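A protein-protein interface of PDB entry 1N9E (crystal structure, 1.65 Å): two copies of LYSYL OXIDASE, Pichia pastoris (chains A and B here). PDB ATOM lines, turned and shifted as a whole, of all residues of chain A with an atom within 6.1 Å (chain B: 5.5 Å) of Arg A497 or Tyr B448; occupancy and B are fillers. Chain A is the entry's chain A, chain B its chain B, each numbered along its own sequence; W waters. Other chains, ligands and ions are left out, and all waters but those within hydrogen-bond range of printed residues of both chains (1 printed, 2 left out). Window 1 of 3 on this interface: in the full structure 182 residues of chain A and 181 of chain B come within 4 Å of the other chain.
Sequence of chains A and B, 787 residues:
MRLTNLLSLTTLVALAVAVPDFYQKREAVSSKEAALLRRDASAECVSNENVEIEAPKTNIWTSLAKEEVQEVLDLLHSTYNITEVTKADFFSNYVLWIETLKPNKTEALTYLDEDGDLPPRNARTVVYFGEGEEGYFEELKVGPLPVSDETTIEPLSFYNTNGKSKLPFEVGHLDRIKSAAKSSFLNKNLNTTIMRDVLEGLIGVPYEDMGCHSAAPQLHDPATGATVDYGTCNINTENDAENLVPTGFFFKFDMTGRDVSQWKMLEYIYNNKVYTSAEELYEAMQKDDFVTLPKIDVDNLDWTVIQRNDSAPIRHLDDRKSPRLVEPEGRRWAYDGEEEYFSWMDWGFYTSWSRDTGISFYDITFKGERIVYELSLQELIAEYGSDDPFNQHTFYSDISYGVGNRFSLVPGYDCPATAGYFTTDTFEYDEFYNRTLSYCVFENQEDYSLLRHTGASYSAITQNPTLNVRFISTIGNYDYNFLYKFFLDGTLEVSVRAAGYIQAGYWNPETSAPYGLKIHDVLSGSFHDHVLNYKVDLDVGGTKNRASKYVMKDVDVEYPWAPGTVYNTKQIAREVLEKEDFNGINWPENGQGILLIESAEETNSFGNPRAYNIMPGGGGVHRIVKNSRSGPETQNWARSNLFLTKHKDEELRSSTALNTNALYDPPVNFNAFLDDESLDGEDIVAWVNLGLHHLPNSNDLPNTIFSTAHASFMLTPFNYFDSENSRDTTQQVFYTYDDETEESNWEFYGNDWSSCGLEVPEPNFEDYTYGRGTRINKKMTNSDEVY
Ser B449 touches Tyr A413 (CB to O, 3.9 Å).
Tyr A413 touches Gln B463.
Arg A470 touches Tyr B448.
CZ of Tyr B448 touches CZ of Arg A497, at 3.3 Å.
CD2 of Tyr B448 touches CB of Phe A706, 3.9 Å away.
CD1 of Phe A706 touches O of Ser B449 (3.2 Å).
CA of Ser A707 touches OH of Tyr B448 (3.6 Å).
Leu B450 touches Ser A707 (CD1 to OG, 3.5 Å).
Ser A707 touches Phe B487 (CB to CE1, 3.996 Å).
Water W1 lies within hydrogen-bond range of the side-chain carboxylate (OD1) of Asp A414 (2.8 Å) and the side-chain hydroxyl (OG) of Ser B449 (2.8 Å).
No position is printed for both chains.
Of the 11 pairs that touch across the chains among the printed residues, none has its exchanged pair printed and touching as well.
Arg A497 touches one residue of chain B.
Tyr B448 touches four residues of chain A.
Printed residues of chain A within 4 Å of Ser B449: Tyr A413 (3.9 Å) and Phe A706 (3.2 Å).
Of the printed residues of chain A, Phe B487 touches Ser A707 (3.996 Å).
Printed residues of chain B within 4 Å of Tyr A413: Ser B449 and Gln B463.
Of the printed residues of chain B, Arg A470 touches Asp B447 (2.8 Å) and Tyr B448 (3.4 Å).
Of the printed residues of chain B, Phe A706 touches Tyr B448, Ser B449 and Leu B450.
Asn B464 touches none of the printed residues of chain A.
Asp A479 touches none of the printed residues of chain B.
The side-chain amide nitrogen (ND2) of Asn B464 lies close to the side-chain hydroxyl (OH) of Tyr B448 (3.2 Å).
O of Ser A707 is in hydrogen-bond range of NH1 of Arg A497, 3.3 Å away.
The guanidinium group (NH1) of Arg A497 lies within hydrogen-bond range of the backbone carbonyl oxygen (O) of Phe A706 (2.9 Å).
The backbone carbonyl oxygen (O) of Arg A497 is in hydrogen-bond range of the backbone NH (N) of Asn A481, at 2.8 Å.
NE of Arg A470 sits at hydrogen-bond distance from OD1 of Asn A481, at 2.8 Å.
The guanidinium group of Arg A470 lies within hydrogen-bond range of the backbone carbonyl oxygen of Asp A414, 2.8 Å away.
NH1 of Arg A470 is in hydrogen-bond range of O of Asp B447 (2.8 Å).
O of Leu B450 sits at hydrogen-bond distance from N of Phe A706.
Hydrophobic or aromatic side chains of chain B that line the printed part of chain A: Tyr B448, Leu B450 and Phe B487.
Hydrophobic or aromatic side chains of chain A that line the printed part of chain B: Tyr A413 and Phe A706.
Along chain A the printed residues that touch a printed residue of chain B span positions 413 to 707.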
ATOM      1  N   TYR A 413      18.770 -29.370  10.489  1.00  0.00           N
ATOM      2  CA  TYR A 413      17.455 -29.004   9.995  1.00  0.00           C
ATOM      3  C   TYR A 413      16.342 -29.180  11.023  1.00  0.00           C
ATOM      4  O   TYR A 413      15.587 -28.247  11.291  1.00  0.00           O
ATOM      5  CB  TYR A 413      17.144 -29.814   8.748  1.00  0.00           C
ATOM      6  CG  TYR A 413      18.025 -29.438   7.596  1.00  0.00           C
ATOM      7  CD1 TYR A 413      19.277 -30.028   7.420  1.00  0.00           C
ATOM      8  CD2 TYR A 413      17.602 -28.484   6.676  1.00  0.00           C
ATOM      9  CE1 TYR A 413      20.094 -29.661   6.328  1.00  0.00           C
ATOM     10  CE2 TYR A 413      18.402 -28.118   5.603  1.00  0.00           C
ATOM     11  CZ  TYR A 413      19.637 -28.707   5.437  1.00  0.00           C
ATOM     12  OH  TYR A 413      20.399 -28.328   4.368  1.00  0.00           O
ATOM     13  N   ASP A 414      16.230 -30.373  11.600  1.00  0.00           N
ATOM     14  CA  ASP A 414      15.174 -30.572  12.581  1.00  0.00           C
ATOM     15  C   ASP A 414      15.478 -29.847  13.894  1.00  0.00           C
ATOM     16  O   ASP A 414      14.577 -29.489  14.656  1.00  0.00           O
ATOM     17  CB  ASP A 414      15.021 -32.058  12.882  1.00  0.00           C
ATOM     18  CG  ASP A 414      14.252 -32.800  11.816  1.00  0.00           C
ATOM     19  OD1 ASP A 414      13.444 -32.184  11.092  1.00  0.00           O
ATOM     20  OD2 ASP A 414      14.402 -34.027  11.639  1.00  0.00           O
ATOM     21  N   ARG A 470      13.369 -30.890  22.013  1.00  0.00           N
ATOM     22  CA  ARG A 470      12.480 -31.275  20.910  1.00  0.00           C
ATOM     23  C   ARG A 470      12.581 -32.746  20.563  1.00  0.00           C
ATOM     24  O   ARG A 470      13.659 -33.349  20.647  1.00  0.00           O
ATOM     25  CB  ARG A 470      12.824 -30.466  19.635  1.00  0.00           C
ATOM     26  CG  ARG A 470      12.325 -31.068  18.301  1.00  0.00           C
ATOM     27  CD  ARG A 470      12.528 -30.172  17.033  1.00  0.00           C
ATOM     28  NE  ARG A 470      11.831 -28.900  17.196  1.00  0.00           N
ATOM     29  CZ  ARG A 470      12.375 -27.705  16.978  1.00  0.00           C
ATOM     30  NH1 ARG A 470      13.642 -27.614  16.582  1.00  0.00           N
ATOM     31  NH2 ARG A 470      11.649 -26.608  17.163  1.00  0.00           N
ATOM     32  N   ASP A 479       3.736 -35.703  10.589  1.00  0.00           N
ATOM     33  CA  ASP A 479       5.014 -35.381  11.281  1.00  0.00           C
ATOM     34  C   ASP A 479       4.695 -34.447  12.423  1.00  0.00           C
ATOM     35  O   ASP A 479       4.314 -33.305  12.177  1.00  0.00           O
ATOM     36  CB  ASP A 479       6.021 -34.696  10.312  1.00  0.00           C
ATOM     37  CG  ASP A 479       6.460 -35.611   9.199  1.00  0.00           C
ATOM     38  OD1 ASP A 479       5.636 -35.884   8.305  1.00  0.00           O
ATOM     39  OD2 ASP A 479       7.607 -36.110   9.136  1.00  0.00           O
ATOM     40  N   TYR A 480       4.846 -34.919  13.665  1.00  0.00           N
ATOM     41  CA  TYR A 480       4.527 -34.090  14.820  1.00  0.00           C
ATOM     42  C   TYR A 480       5.784 -33.559  15.482  1.00  0.00           C
ATOM     43  O   TYR A 480       6.664 -34.337  15.845  1.00  0.00           O
ATOM     44  CB  TYR A 480       3.717 -34.897  15.841  1.00  0.00           C
ATOM     45  CG  TYR A 480       2.362 -35.298  15.297  1.00  0.00           C
ATOM     46  CD1 TYR A 480       1.338 -34.372  15.211  1.00  0.00           C
ATOM     47  CD2 TYR A 480       2.120 -36.602  14.869  1.00  0.00           C
ATOM     48  CE1 TYR A 480       0.101 -34.710  14.720  1.00  0.00           C
ATOM     49  CE2 TYR A 480       0.855 -36.962  14.364  1.00  0.00           C
ATOM     50  CZ  TYR A 480      -0.144 -35.993  14.298  1.00  0.00           C
ATOM     51  OH  TYR A 480      -1.406 -36.281  13.813  1.00  0.00           O
ATOM     52  N   ASN A 481       5.862 -32.242  15.644  1.00  0.00           N
ATOM     53  CA  ASN A 481       7.064 -31.598  16.174  1.00  0.00           C
ATOM     54  C   ASN A 481       6.758 -31.049  17.560  1.00  0.00           C
ATOM     55  O   ASN A 481       6.018 -30.089  17.692  1.00  0.00           O
ATOM     56  CB  ASN A 481       7.453 -30.497  15.181  1.00  0.00           C
ATOM     57  CG  ASN A 481       8.773 -29.813  15.511  1.00  0.00           C
ATOM     58  OD1 ASN A 481       9.194 -29.740  16.658  1.00  0.00           O
ATOM     59  ND2 ASN A 481       9.431 -29.302  14.470  1.00  0.00           N
ATOM     60  N   PHE A 482       7.337 -31.673  18.581  1.00  0.00           N
ATOM     61  CA  PHE A 482       7.073 -31.312  19.969  1.00  0.00           C
ATOM     62  C   PHE A 482       8.218 -30.495  20.543  1.00  0.00           C
ATOM     63  O   PHE A 482       9.379 -30.868  20.385  1.00  0.00           O
ATOM     64  CB  PHE A 482       6.956 -32.574  20.795  1.00  0.00           C
ATOM     65  CG  PHE A 482       5.907 -33.524  20.318  1.00  0.00           C
ATOM     66  CD1 PHE A 482       6.261 -34.653  19.600  1.00  0.00           C
ATOM     67  CD2 PHE A 482       4.574 -33.290  20.591  1.00  0.00           C
ATOM     68  CE1 PHE A 482       5.289 -35.542  19.157  1.00  0.00           C
ATOM     69  CE2 PHE A 482       3.594 -34.181  20.149  1.00  0.00           C
ATOM     70  CZ  PHE A 482       3.959 -35.295  19.436  1.00  0.00           C
ATOM     71  N   LEU A 483       7.892 -29.392  21.205  1.00  0.00           N
ATOM     72  CA  LEU A 483       8.922 -28.514  21.741  1.00  0.00           C
ATOM     73  C   LEU A 483       8.573 -28.111  23.152  1.00  0.00           C
ATOM     74  O   LEU A 483       7.423 -27.829  23.459  1.00  0.00           O
ATOM     75  CB  LEU A 483       9.037 -27.256  20.871  1.00  0.00           C
ATOM     76  CG  LEU A 483      10.192 -26.298  21.223  1.00  0.00           C
ATOM     77  CD1 LEU A 483      11.546 -26.962  20.953  1.00  0.00           C
ATOM     78  CD2 LEU A 483      10.048 -24.998  20.435  1.00  0.00           C
ATOM     79  N   SER A 495       4.605 -26.904  23.354  1.00  0.00           N
ATOM     80  CA  SER A 495       3.968 -26.697  22.059  1.00  0.00           C
ATOM     81  C   SER A 495       4.106 -27.851  21.098  1.00  0.00           C
ATOM     82  O   SER A 495       4.945 -28.726  21.255  1.00  0.00           O
ATOM     83  CB  SER A 495       4.562 -25.462  21.373  1.00  0.00           C
ATOM     84  OG  SER A 495       5.929 -25.675  21.019  1.00  0.00           O
ATOM     85  N   VAL A 496       3.259 -27.833  20.086  1.00  0.00           N
ATOM     86  CA  VAL A 496       3.348 -28.797  19.022  1.00  0.00           C
ATOM     87  C   VAL A 496       3.113 -28.074  17.709  1.00  0.00           C
ATOM     88  O   VAL A 496       2.367 -27.086  17.647  1.00  0.00           O
ATOM     89  CB  VAL A 496       2.319 -29.934  19.228  1.00  0.00           C
ATOM     90  CG1 VAL A 496       0.857 -29.397  19.172  1.00  0.00           C
ATOM     91  CG2 VAL A 496       2.519 -31.079  18.222  1.00  0.00           C
ATOM     92  N   ARG A 497       3.754 -28.567  16.663  1.00  0.00           N
ATOM     93  CA  ARG A 497       3.455 -28.118  15.315  1.00  0.00           C
ATOM     94  C   ARG A 497       3.316 -29.377  14.496  1.00  0.00           C
ATOM     95  O   ARG A 497       4.020 -30.356  14.740  1.00  0.00           O
ATOM     96  CB  ARG A 497       4.606 -27.289  14.768  1.00  0.00           C
ATOM     97  CG  ARG A 497       4.800 -25.944  15.469  1.00  0.00           C
ATOM     98  CD  ARG A 497       6.011 -25.177  14.936  1.00  0.00           C
ATOM     99  NE  ARG A 497       6.214 -23.896  15.626  1.00  0.00           N
ATOM    100  CZ  ARG A 497       5.577 -22.781  15.310  1.00  0.00           C
ATOM    101  NH1 ARG A 497       4.688 -22.787  14.312  1.00  0.00           N
ATOM    102  NH2 ARG A 497       5.826 -21.651  15.992  1.00  0.00           N
ATOM    103  N   ALA A 498       2.414 -29.356  13.523  1.00  0.00           N
ATOM    104  CA  ALA A 498       2.192 -30.536  12.699  1.00  0.00           C
ATOM    105  C   ALA A 498       2.485 -30.285  11.215  1.00  0.00           C
ATOM    106  O   ALA A 498       2.355 -29.166  10.713  1.00  0.00           O
ATOM    107  CB  ALA A 498       0.789 -31.052  12.896  1.00  0.00           C
ATOM    108  N   ALA A 499       2.892 -31.333  10.511  1.00  0.00           N
ATOM    109  CA  ALA A 499       3.161 -31.224   9.076  1.00  0.00           C
ATOM    110  C   ALA A 499       3.072 -32.618   8.482  1.00  0.00           C
ATOM    111  O   ALA A 499       2.606 -33.550   9.133  1.00  0.00           O
ATOM    112  CB  ALA A 499       4.541 -30.650   8.819  1.00  0.00           C
ATOM    113  N   LEU A 692      -6.020 -28.743  16.889  1.00  0.00           N
ATOM    114  CA  LEU A 692      -6.154 -28.055  15.607  1.00  0.00           C
ATOM    115  C   LEU A 692      -7.411 -28.547  14.907  1.00  0.00           C
ATOM    116  O   LEU A 692      -7.636 -29.774  14.850  1.00  0.00           O
ATOM    117  CB  LEU A 692      -4.975 -28.395  14.708  1.00  0.00           C
ATOM    118  CG  LEU A 692      -3.595 -27.996  15.207  1.00  0.00           C
ATOM    119  CD1 LEU A 692      -2.542 -28.743  14.396  1.00  0.00           C
ATOM    120  CD2 LEU A 692      -3.433 -26.492  15.133  1.00  0.00           C
ATOM    121  N   PHE A 706       4.489 -26.334   9.143  1.00  0.00           N
ATOM    122  CA  PHE A 706       4.541 -26.258  10.599  1.00  0.00           C
ATOM    123  C   PHE A 706       4.223 -24.848  11.121  1.00  0.00           C
ATOM    124  O   PHE A 706       3.806 -24.669  12.269  1.00  0.00           O
ATOM    125  CB  PHE A 706       5.974 -26.545  11.057  1.00  0.00           C
ATOM    126  CG  PHE A 706       6.369 -28.009  11.159  1.00  0.00           C
ATOM    127  CD1 PHE A 706       7.581 -28.431  10.617  1.00  0.00           C
ATOM    128  CD2 PHE A 706       5.573 -28.950  11.789  1.00  0.00           C
ATOM    129  CE1 PHE A 706       7.980 -29.753  10.696  1.00  0.00           C
ATOM    130  CE2 PHE A 706       5.972 -30.284  11.875  1.00  0.00           C
ATOM    131  CZ  PHE A 706       7.172 -30.681  11.328  1.00  0.00           C
ATOM    132  N   SER A 707       4.429 -23.838  10.288  1.00  0.00           N
ATOM    133  CA  SER A 707       4.263 -22.466  10.763  1.00  0.00           C
ATOM    134  C   SER A 707       2.819 -22.141  11.143  1.00  0.00           C
ATOM    135  O   SER A 707       2.569 -21.426  12.126  1.00  0.00           O
ATOM    136  CB  SER A 707       4.708 -21.503   9.674  1.00  0.00           C
ATOM    137  OG  SER A 707       4.074 -21.892   8.461  1.00  0.00           O
ATOM    138  N   THR A 708       1.866 -22.657  10.377  1.00  0.00           N
ATOM    139  CA  THR A 708       0.472 -22.310  10.633  1.00  0.00           C
ATOM    140  C   THR A 708      -0.336 -23.453  11.229  1.00  0.00           C
ATOM    141  O   THR A 708      -1.558 -23.330  11.351  1.00  0.00           O
ATOM    142  CB  THR A 708      -0.197 -21.832   9.328  1.00  0.00           C
ATOM    143  OG1 THR A 708       0.113 -22.750   8.247  1.00  0.00           O
ATOM    144  CG2 THR A 708       0.414 -20.531   8.890  1.00  0.00           C
ATOM    145  N   ALA A 709       0.320 -24.557  11.586  1.00  0.00           N
ATOM    146  CA  ALA A 709      -0.362 -25.682  12.254  1.00  0.00           C
ATOM    147  C   ALA A 709       0.317 -25.791  13.623  1.00  0.00           C
ATOM    148  O   ALA A 709       1.134 -26.668  13.852  1.00  0.00           O
ATOM    149  CB  ALA A 709      -0.237 -26.979  11.457  1.00  0.00           C
ATOM    150  N   HIS A 710      -0.043 -24.876  14.516  1.00  0.00           N
ATOM    151  CA  HIS A 710       0.668 -24.691  15.781  1.00  0.00           C
ATOM    152  C   HIS A 710      -0.262 -24.561  16.982  1.00  0.00           C
ATOM    153  O   HIS A 710      -1.295 -23.911  16.894  1.00  0.00           O
ATOM    154  CB  HIS A 710       1.454 -23.385  15.587  1.00  0.00           C
ATOM    155  CG  HIS A 710       2.232 -22.885  16.765  1.00  0.00           C
ATOM    156  ND1 HIS A 710       3.028 -23.681  17.562  1.00  0.00           N
ATOM    157  CD2 HIS A 710       2.338 -21.632  17.267  1.00  0.00           C
ATOM    158  CE1 HIS A 710       3.585 -22.939  18.507  1.00  0.00           C
ATOM    159  NE2 HIS A 710       3.181 -21.694  18.349  1.00  0.00           N
ATOM    160  N   ALA A 711       0.112 -25.183  18.103  1.00  0.00           N
ATOM    161  CA  ALA A 711      -0.683 -25.049  19.338  1.00  0.00           C
ATOM    162  C   ALA A 711       0.295 -24.982  20.481  1.00  0.00           C
ATOM    163  O   ALA A 711       1.372 -25.587  20.408  1.00  0.00           O
ATOM    164  CB  ALA A 711      -1.635 -26.239  19.518  1.00  0.00           C
ATOM    165  N   GLU B 446      14.184 -19.329  12.090  1.00  0.00           N
ATOM    166  CA  GLU B 446      13.296 -19.792  13.157  1.00  0.00           C
ATOM    167  C   GLU B 446      13.827 -21.125  13.679  1.00  0.00           C
ATOM    168  O   GLU B 446      14.522 -21.861  12.959  1.00  0.00           O
ATOM    169  CB  GLU B 446      11.843 -19.953  12.662  1.00  0.00           C
ATOM    170  CG  GLU B 446      11.207 -18.679  12.093  1.00  0.00           C
ATOM    171  CD  GLU B 446      11.149 -17.543  13.104  1.00  0.00           C
ATOM    172  OE1 GLU B 446      11.327 -16.383  12.681  1.00  0.00           O
ATOM    173  OE2 GLU B 446      10.926 -17.798  14.309  1.00  0.00           O
ATOM    174  N   ASP B 447      13.505 -21.455  14.923  1.00  0.00           N
ATOM    175  CA  ASP B 447      14.113 -22.636  15.502  1.00  0.00           C
ATOM    176  C   ASP B 447      13.341 -23.919  15.243  1.00  0.00           C
ATOM    177  O   ASP B 447      13.570 -24.928  15.914  1.00  0.00           O
ATOM    178  CB  ASP B 447      14.407 -22.439  17.003  1.00  0.00           C
ATOM    179  CG  ASP B 447      13.153 -22.358  17.862  1.00  0.00           C
ATOM    180  OD1 ASP B 447      12.026 -22.495  17.331  1.00  0.00           O
ATOM    181  OD2 ASP B 447      13.208 -22.160  19.098  1.00  0.00           O
ATOM    182  N   TYR B 448      12.435 -23.868  14.277  1.00  0.00           N
ATOM    183  CA  TYR B 448      11.692 -25.061  13.837  1.00  0.00           C
ATOM    184  C   TYR B 448      11.675 -24.950  12.317  1.00  0.00           C
ATOM    185  O   TYR B 448      11.704 -23.844  11.762  1.00  0.00           O
ATOM    186  CB  TYR B 448      10.248 -25.117  14.398  1.00  0.00           C
ATOM    187  CG  TYR B 448       9.389 -23.980  13.906  1.00  0.00           C
ATOM    188  CD1 TYR B 448       9.454 -22.717  14.519  1.00  0.00           C
ATOM    189  CD2 TYR B 448       8.521 -24.152  12.836  1.00  0.00           C
ATOM    190  CE1 TYR B 448       8.661 -21.657  14.060  1.00  0.00           C
ATOM    191  CE2 TYR B 448       7.729 -23.102  12.377  1.00  0.00           C
ATOM    192  CZ  TYR B 448       7.808 -21.867  12.994  1.00  0.00           C
ATOM    193  OH  TYR B 448       7.018 -20.848  12.518  1.00  0.00           O
ATOM    194  N   SER B 449      11.627 -26.081  11.635  1.00  0.00           N
ATOM    195  CA  SER B 449      11.630 -26.067  10.176  1.00  0.00           C
ATOM    196  C   SER B 449      10.255 -25.648   9.620  1.00  0.00           C
ATOM    197  O   SER B 449       9.233 -25.728  10.306  1.00  0.00           O
ATOM    198  CB  SER B 449      12.099 -27.444   9.646  1.00  0.00           C
ATOM    199  OG  SER B 449      11.010 -28.350   9.483  1.00  0.00           O
ATOM    200  N   LEU B 450      10.216 -25.199   8.368  1.00  0.00           N
ATOM    201  CA  LEU B 450       8.927 -24.818   7.784  1.00  0.00           C
ATOM    202  C   LEU B 450       8.010 -26.017   7.528  1.00  0.00           C
ATOM    203  O   LEU B 450       6.799 -25.931   7.740  1.00  0.00           O
ATOM    204  CB  LEU B 450       9.116 -24.013   6.502  1.00  0.00           C
ATOM    205  CG  LEU B 450       7.870 -23.397   5.856  1.00  0.00           C
ATOM    206  CD1 LEU B 450       7.100 -22.488   6.853  1.00  0.00           C
ATOM    207  CD2 LEU B 450       8.283 -22.601   4.617  1.00  0.00           C
ATOM    208  N   GLN B 463      13.861 -25.466   5.627  1.00  0.00           N
ATOM    209  CA  GLN B 463      14.134 -24.532   6.705  1.00  0.00           C
ATOM    210  C   GLN B 463      13.130 -23.365   6.704  1.00  0.00           C
ATOM    211  O   GLN B 463      12.375 -23.154   5.756  1.00  0.00           O
ATOM    212  CB  GLN B 463      15.543 -23.967   6.529  1.00  0.00           C
ATOM    213  CG  GLN B 463      16.648 -25.038   6.615  1.00  0.00           C
ATOM    214  CD  GLN B 463      18.000 -24.387   6.550  1.00  0.00           C
ATOM    215  OE1 GLN B 463      18.553 -23.998   7.581  1.00  0.00           O
ATOM    216  NE2 GLN B 463      18.533 -24.261   5.356  1.00  0.00           N
ATOM    217  N   ASN B 464      13.148 -22.599   7.787  1.00  0.00           N
ATOM    218  CA  ASN B 464      12.201 -21.517   7.998  1.00  0.00           C
ATOM    219  C   ASN B 464      12.893 -20.186   8.289  1.00  0.00           C
ATOM    220  O   ASN B 464      12.787 -19.659   9.390  1.00  0.00           O
ATOM    221  CB  ASN B 464      11.333 -21.918   9.190  1.00  0.00           C
ATOM    222  CG  ASN B 464      10.039 -21.133   9.293  1.00  0.00           C
ATOM    223  OD1 ASN B 464       9.656 -20.369   8.397  1.00  0.00           O
ATOM    224  ND2 ASN B 464       9.344 -21.330  10.419  1.00  0.00           N
ATOM    225  N   PHE B 487       7.088 -15.002   5.781  1.00  0.00           N
ATOM    226  CA  PHE B 487       7.519 -16.376   5.580  1.00  0.00           C
ATOM    227  C   PHE B 487       7.628 -16.761   4.099  1.00  0.00           C
ATOM    228  O   PHE B 487       7.060 -16.112   3.226  1.00  0.00           O
ATOM    229  CB  PHE B 487       6.526 -17.348   6.219  1.00  0.00           C
ATOM    230  CG  PHE B 487       6.389 -17.239   7.729  1.00  0.00           C
ATOM    231  CD1 PHE B 487       6.959 -18.201   8.536  1.00  0.00           C
ATOM    232  CD2 PHE B 487       5.688 -16.202   8.317  1.00  0.00           C
ATOM    233  CE1 PHE B 487       6.852 -18.140   9.929  1.00  0.00           C
ATOM    234  CE2 PHE B 487       5.568 -16.125   9.727  1.00  0.00           C
ATOM    235  CZ  PHE B 487       6.147 -17.086  10.526  1.00  0.00           C
HETATM  236  O   HOH W   1      11.545 -30.213  11.505  1.00  0.00           O
